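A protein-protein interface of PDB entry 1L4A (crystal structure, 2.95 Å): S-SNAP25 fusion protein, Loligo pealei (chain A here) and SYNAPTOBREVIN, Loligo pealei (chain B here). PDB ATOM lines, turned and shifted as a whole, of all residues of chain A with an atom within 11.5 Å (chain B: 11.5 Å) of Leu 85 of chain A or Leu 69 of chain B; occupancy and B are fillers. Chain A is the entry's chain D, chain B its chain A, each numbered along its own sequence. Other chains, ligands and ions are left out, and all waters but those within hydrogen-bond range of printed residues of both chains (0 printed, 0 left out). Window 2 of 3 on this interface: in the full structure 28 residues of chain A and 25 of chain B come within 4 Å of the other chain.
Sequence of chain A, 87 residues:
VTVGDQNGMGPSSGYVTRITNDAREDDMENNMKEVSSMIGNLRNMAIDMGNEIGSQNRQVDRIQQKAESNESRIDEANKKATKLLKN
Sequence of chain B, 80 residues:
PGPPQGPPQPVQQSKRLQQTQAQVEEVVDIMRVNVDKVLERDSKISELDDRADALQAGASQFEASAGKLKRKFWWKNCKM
Printed residues of chain B within 4 Å of Asn 78 of chain A: Gln 61, Phe 62 and Ser 65. Lys 80 of chain A touches none of the printed residues of chain B. Ala 81 of chain A touches one residue of chain B. No residue of chain B comes within 4 Å of Leu 84 of chain A. Leu 85 of chain A touches just one residue of chain B: Leu 69. Of the printed residues of chain A, Gln 61 of chain B touches Asn 78 (2.9 Å). Of the printed residues of chain A, Phe 62 of chain B touches Ala 77 (3.3 Å) and Asn 78 (3.1 Å). No residue of chain A comes within 4 Å of Ala 64 of chain B. Ser 65 of chain B touches just these residues of chain A: Asn 78 (3.4 Å) and Ala 81 (3.4 Å). No residue of chain A comes within 4 Å of Ala 66 of chain B. No residue of chain A comes within 4 Å of Gly 67 of chain B. Lys 68 of chain B touches none of the printed residues of chain A. Of the printed residues of chain A, Leu 69 of chain B touches Leu 85. No residue of chain A comes within 4 Å of Lys 70 of chain B. No residue of chain A comes within 4 Å of Arg 71 of chain B. No residue of chain A comes within 4 Å of Lys 72 of chain B. No residue of chain A comes within 4 Å of Phe 73 of chain B. No residue of chain A comes within 4 Å of Trp 74 of chain B. The nearest residue of chain A that does not touch Leu 69 of chain B is Leu 84 of chain A (4.8 Å).
O of Gln 61 of chain B lies within hydrogen-bond range of ND2 of Asn 78 of chain A (2.9 Å).
Among the printed residues, merely in contact across the chains: Asn 78 of chain A with Phe 62 of chain B, Leu 85 of chain A with Leu 69 of chain B, Ala 77 of chain A with Phe 62 of chain B, Ala 81 of chain A with Ser 65 of chain B and Asn 78 of chain A with Ser 65 of chain B.
Hydrophobic or aromatic side chains of chain B within 4 Å of the printed part of chain A: Phe 62 and Leu 69. Along chain B the printed residues that touch a printed residue of chain A span positions 61 to 69. Along chain A the printed residues that touch a printed residue of chain B span positions 77 to 85. Among the printed residues, 6 pairs touch across the chains. Among the printed residues, no Asp or Glu carboxylate lies within 4 Å of a Lys or Arg side-chain nitrogen of the other chain.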
ATOM      1  N   ALA A  77       6.863 -27.796  -9.043  1.00  0.00           N
ATOM      2  CA  ALA A  77       5.453 -28.141  -8.909  1.00  0.00           C
ATOM      3  C   ALA A  77       4.760 -27.847 -10.236  1.00  0.00           C
ATOM      4  O   ALA A  77       3.647 -28.310 -10.475  1.00  0.00           O
ATOM      5  CB  ALA A  77       4.808 -27.342  -7.780  1.00  0.00           C
ATOM      6  N   ASN A  78       5.418 -27.070 -11.096  1.00  0.00           N
ATOM      7  CA  ASN A  78       4.861 -26.759 -12.409  1.00  0.00           C
ATOM      8  C   ASN A  78       5.113 -27.932 -13.346  1.00  0.00           C
ATOM      9  O   ASN A  78       4.567 -27.998 -14.451  1.00  0.00           O
ATOM     10  CB  ASN A  78       5.489 -25.499 -12.993  1.00  0.00           C
ATOM     11  CG  ASN A  78       5.109 -25.290 -14.442  1.00  0.00           C
ATOM     12  OD1 ASN A  78       5.599 -25.989 -15.326  1.00  0.00           O
ATOM     13  ND2 ASN A  78       4.217 -24.341 -14.694  1.00  0.00           N
ATOM     14  N   LYS A  79       5.959 -28.853 -12.894  1.00  0.00           N
ATOM     15  CA  LYS A  79       6.265 -30.047 -13.663  1.00  0.00           C
ATOM     16  C   LYS A  79       4.952 -30.819 -13.712  1.00  0.00           C
ATOM     17  O   LYS A  79       4.544 -31.315 -14.760  1.00  0.00           O
ATOM     18  CB  LYS A  79       7.341 -30.867 -12.957  1.00  0.00           C
ATOM     19  N   LYS A  80       4.288 -30.892 -12.561  1.00  0.00           N
ATOM     20  CA  LYS A  80       3.010 -31.582 -12.440  1.00  0.00           C
ATOM     21  C   LYS A  80       1.962 -30.928 -13.341  1.00  0.00           C
ATOM     22  O   LYS A  80       1.007 -31.574 -13.762  1.00  0.00           O
ATOM     23  CB  LYS A  80       2.532 -31.543 -10.987  1.00  0.00           C
ATOM     24  CG  LYS A  80       3.514 -32.126  -9.975  1.00  0.00           C
ATOM     25  CD  LYS A  80       3.620 -33.633 -10.094  1.00  0.00           C
ATOM     26  CE  LYS A  80       4.469 -34.205  -8.976  1.00  0.00           C
ATOM     27  NZ  LYS A  80       4.486 -35.694  -9.016  1.00  0.00           N
ATOM     28  N   ALA A  81       2.144 -29.641 -13.624  1.00  0.00           N
ATOM     29  CA  ALA A  81       1.218 -28.907 -14.482  1.00  0.00           C
ATOM     30  C   ALA A  81       1.447 -29.342 -15.920  1.00  0.00           C
ATOM     31  O   ALA A  81       0.589 -29.156 -16.784  1.00  0.00           O
ATOM     32  CB  ALA A  81       1.447 -27.406 -14.343  1.00  0.00           C
ATOM     33  N   THR A  82       2.620 -29.916 -16.168  1.00  0.00           N
ATOM     34  CA  THR A  82       2.978 -30.408 -17.494  1.00  0.00           C
ATOM     35  C   THR A  82       2.591 -31.889 -17.588  1.00  0.00           C
ATOM     36  O   THR A  82       2.227 -32.384 -18.658  1.00  0.00           O
ATOM     37  CB  THR A  82       4.473 -30.232 -17.730  1.00  0.00           C
ATOM     38  N   LYS A  83       2.667 -32.584 -16.456  1.00  0.00           N
ATOM     39  CA  LYS A  83       2.316 -33.996 -16.386  1.00  0.00           C
ATOM     40  C   LYS A  83       0.806 -34.164 -16.541  1.00  0.00           C
ATOM     41  O   LYS A  83       0.332 -34.643 -17.572  1.00  0.00           O
ATOM     42  CB  LYS A  83       2.763 -34.589 -15.046  1.00  0.00           C
ATOM     43  CG  LYS A  83       2.397 -36.056 -14.856  1.00  0.00           C
ATOM     44  CD  LYS A  83       2.723 -36.531 -13.447  1.00  0.00           C
ATOM     45  CE  LYS A  83       2.270 -37.967 -13.230  1.00  0.00           C
ATOM     46  NZ  LYS A  83       2.541 -38.440 -11.842  1.00  0.00           N
ATOM     47  N   LEU A  84       0.056 -33.771 -15.512  1.00  0.00           N
ATOM     48  CA  LEU A  84      -1.399 -33.871 -15.531  1.00  0.00           C
ATOM     49  C   LEU A  84      -1.962 -33.440 -16.884  1.00  0.00           C
ATOM     50  O   LEU A  84      -2.390 -34.278 -17.678  1.00  0.00           O
ATOM     51  CB  LEU A  84      -1.992 -33.021 -14.421  1.00  0.00           C
ATOM     52  N   LEU A  85      -1.955 -32.138 -17.150  1.00  0.00           N
ATOM     53  CA  LEU A  85      -2.466 -31.615 -18.415  1.00  0.00           C
ATOM     54  C   LEU A  85      -1.475 -31.835 -19.557  1.00  0.00           C
ATOM     55  O   LEU A  85      -1.874 -32.453 -20.569  1.00  0.00           O
ATOM     56  CB  LEU A  85      -2.777 -30.134 -18.281  1.00  0.00           C
ATOM     57  N   GLN B  61       4.777 -18.851 -15.640  1.00  0.00           N
ATOM     58  CA  GLN B  61       4.809 -20.160 -16.273  1.00  0.00           C
ATOM     59  C   GLN B  61       3.839 -21.082 -15.536  1.00  0.00           C
ATOM     60  O   GLN B  61       3.233 -21.973 -16.133  1.00  0.00           O
ATOM     61  CB  GLN B  61       6.218 -20.730 -16.230  1.00  0.00           C
ATOM     62  N   PHE B  62       3.695 -20.861 -14.234  1.00  0.00           N
ATOM     63  CA  PHE B  62       2.790 -21.660 -13.415  1.00  0.00           C
ATOM     64  C   PHE B  62       1.387 -21.095 -13.605  1.00  0.00           C
ATOM     65  O   PHE B  62       0.410 -21.621 -13.070  1.00  0.00           O
ATOM     66  CB  PHE B  62       3.207 -21.573 -11.944  1.00  0.00           C
ATOM     67  CG  PHE B  62       2.899 -22.810 -11.141  1.00  0.00           C
ATOM     68  CD1 PHE B  62       2.818 -24.057 -11.753  1.00  0.00           C
ATOM     69  CD2 PHE B  62       2.768 -22.738  -9.756  1.00  0.00           C
ATOM     70  CE1 PHE B  62       2.611 -25.215 -10.997  1.00  0.00           C
ATOM     71  CE2 PHE B  62       2.562 -23.892  -8.990  1.00  0.00           C
ATOM     72  CZ  PHE B  62       2.488 -25.131  -9.613  1.00  0.00           C
ATOM     73  N   GLU B  63       1.307 -20.013 -14.375  1.00  0.00           N
ATOM     74  CA  GLU B  63       0.040 -19.360 -14.665  1.00  0.00           C
ATOM     75  C   GLU B  63      -0.584 -20.026 -15.877  1.00  0.00           C
ATOM     76  O   GLU B  63      -1.639 -20.646 -15.773  1.00  0.00           O
ATOM     77  CB  GLU B  63       0.257 -17.871 -14.947  1.00  0.00           C
ATOM     78  CG  GLU B  63      -1.021 -17.072 -15.209  1.00  0.00           C
ATOM     79  CD  GLU B  63      -1.434 -17.051 -16.675  1.00  0.00           C
ATOM     80  OE1 GLU B  63      -1.746 -18.119 -17.236  1.00  0.00           O
ATOM     81  OE2 GLU B  63      -1.452 -15.954 -17.271  1.00  0.00           O
ATOM     82  N   ALA B  64       0.074 -19.896 -17.026  1.00  0.00           N
ATOM     83  CA  ALA B  64      -0.415 -20.492 -18.267  1.00  0.00           C
ATOM     84  C   ALA B  64      -0.709 -21.973 -18.055  1.00  0.00           C
ATOM     85  O   ALA B  64      -1.553 -22.543 -18.741  1.00  0.00           O
ATOM     86  CB  ALA B  64       0.615 -20.313 -19.387  1.00  0.00           C
ATOM     87  N   SER B  65      -0.009 -22.580 -17.097  1.00  0.00           N
ATOM     88  CA  SER B  65      -0.182 -23.992 -16.767  1.00  0.00           C
ATOM     89  C   SER B  65      -1.410 -24.184 -15.881  1.00  0.00           C
ATOM     90  O   SER B  65      -1.614 -25.247 -15.295  1.00  0.00           O
ATOM     91  CB  SER B  65       1.065 -24.519 -16.057  1.00  0.00           C
ATOM     92  N   ALA B  66      -2.219 -23.134 -15.788  1.00  0.00           N
ATOM     93  CA  ALA B  66      -3.440 -23.148 -14.999  1.00  0.00           C
ATOM     94  C   ALA B  66      -4.552 -22.554 -15.858  1.00  0.00           C
ATOM     95  O   ALA B  66      -5.683 -23.021 -15.827  1.00  0.00           O
ATOM     96  CB  ALA B  66      -3.253 -22.334 -13.727  1.00  0.00           C
ATOM     97  N   GLY B  67      -4.225 -21.520 -16.627  1.00  0.00           N
ATOM     98  CA  GLY B  67      -5.221 -20.919 -17.496  1.00  0.00           C
ATOM     99  C   GLY B  67      -5.542 -21.932 -18.577  1.00  0.00           C
ATOM    100  O   GLY B  67      -6.672 -22.014 -19.068  1.00  0.00           O
ATOM    101  N   LYS B  68      -4.521 -22.710 -18.936  1.00  0.00           N
ATOM    102  CA  LYS B  68      -4.635 -23.757 -19.945  1.00  0.00           C
ATOM    103  C   LYS B  68      -5.105 -25.028 -19.255  1.00  0.00           C
ATOM    104  O   LYS B  68      -5.925 -25.766 -19.795  1.00  0.00           O
ATOM    105  CB  LYS B  68      -3.288 -23.993 -20.618  1.00  0.00           C
ATOM    106  N   LEU B  69      -4.572 -25.284 -18.061  1.00  0.00           N
ATOM    107  CA  LEU B  69      -4.977 -26.458 -17.295  1.00  0.00           C
ATOM    108  C   LEU B  69      -6.463 -26.296 -17.010  1.00  0.00           C
ATOM    109  O   LEU B  69      -7.257 -27.174 -17.332  1.00  0.00           O
ATOM    110  CB  LEU B  69      -4.206 -26.547 -15.974  1.00  0.00           C
ATOM    111  CG  LEU B  69      -4.612 -27.666 -15.001  1.00  0.00           C
ATOM    112  CD1 LEU B  69      -4.357 -29.022 -15.625  1.00  0.00           C
ATOM    113  CD2 LEU B  69      -3.819 -27.542 -13.710  1.00  0.00           C
ATOM    114  N   LYS B  70      -6.833 -25.163 -16.418  1.00  0.00           N
ATOM    115  CA  LYS B  70      -8.232 -24.884 -16.111  1.00  0.00           C
ATOM    116  C   LYS B  70      -9.055 -25.040 -17.377  1.00  0.00           C
ATOM    117  O   LYS B  70      -9.787 -26.019 -17.533  1.00  0.00           O
ATOM    118  CB  LYS B  70      -8.392 -23.469 -15.563  1.00  0.00           C
ATOM    119  N   ARG B  71      -8.916 -24.072 -18.280  1.00  0.00           N
ATOM    120  CA  ARG B  71      -9.640 -24.065 -19.549  1.00  0.00           C
ATOM    121  C   ARG B  71      -9.811 -25.462 -20.163  1.00  0.00           C
ATOM    122  O   ARG B  71     -10.848 -25.753 -20.767  1.00  0.00           O
ATOM    123  CB  ARG B  71      -8.936 -23.137 -20.539  1.00  0.00           C
ATOM    124  N   LYS B  72      -8.805 -26.323 -19.998  1.00  0.00           N
ATOM    125  CA  LYS B  72      -8.848 -27.682 -20.545  1.00  0.00           C
ATOM    126  C   LYS B  72      -9.850 -28.581 -19.828  1.00  0.00           C
ATOM    127  O   LYS B  72     -11.048 -28.512 -20.106  1.00  0.00           O
ATOM    128  CB  LYS B  72      -7.455 -28.313 -20.506  1.00  0.00           C
ATOM    129  N   PHE B  73      -9.374 -29.420 -18.909  1.00  0.00           N
ATOM    130  CA  PHE B  73     -10.270 -30.326 -18.189  1.00  0.00           C
ATOM    131  C   PHE B  73      -9.819 -30.666 -16.772  1.00  0.00           C
ATOM    132  O   PHE B  73     -10.328 -30.093 -15.809  1.00  0.00           O
ATOM    133  CB  PHE B  73     -10.458 -31.607 -18.992  1.00  0.00           C
ATOM    134  N   TRP B  74      -8.894 -31.619 -16.654  1.00  0.00           N
ATOM    135  CA  TRP B  74      -8.357 -32.049 -15.358  1.00  0.00           C
ATOM    136  C   TRP B  74      -9.387 -32.680 -14.422  1.00  0.00           C
ATOM    137  O   TRP B  74      -8.996 -33.578 -13.642  1.00  0.00           O
ATOM    138  CB  TRP B  74      -7.677 -30.875 -14.660  1.00  0.00           C
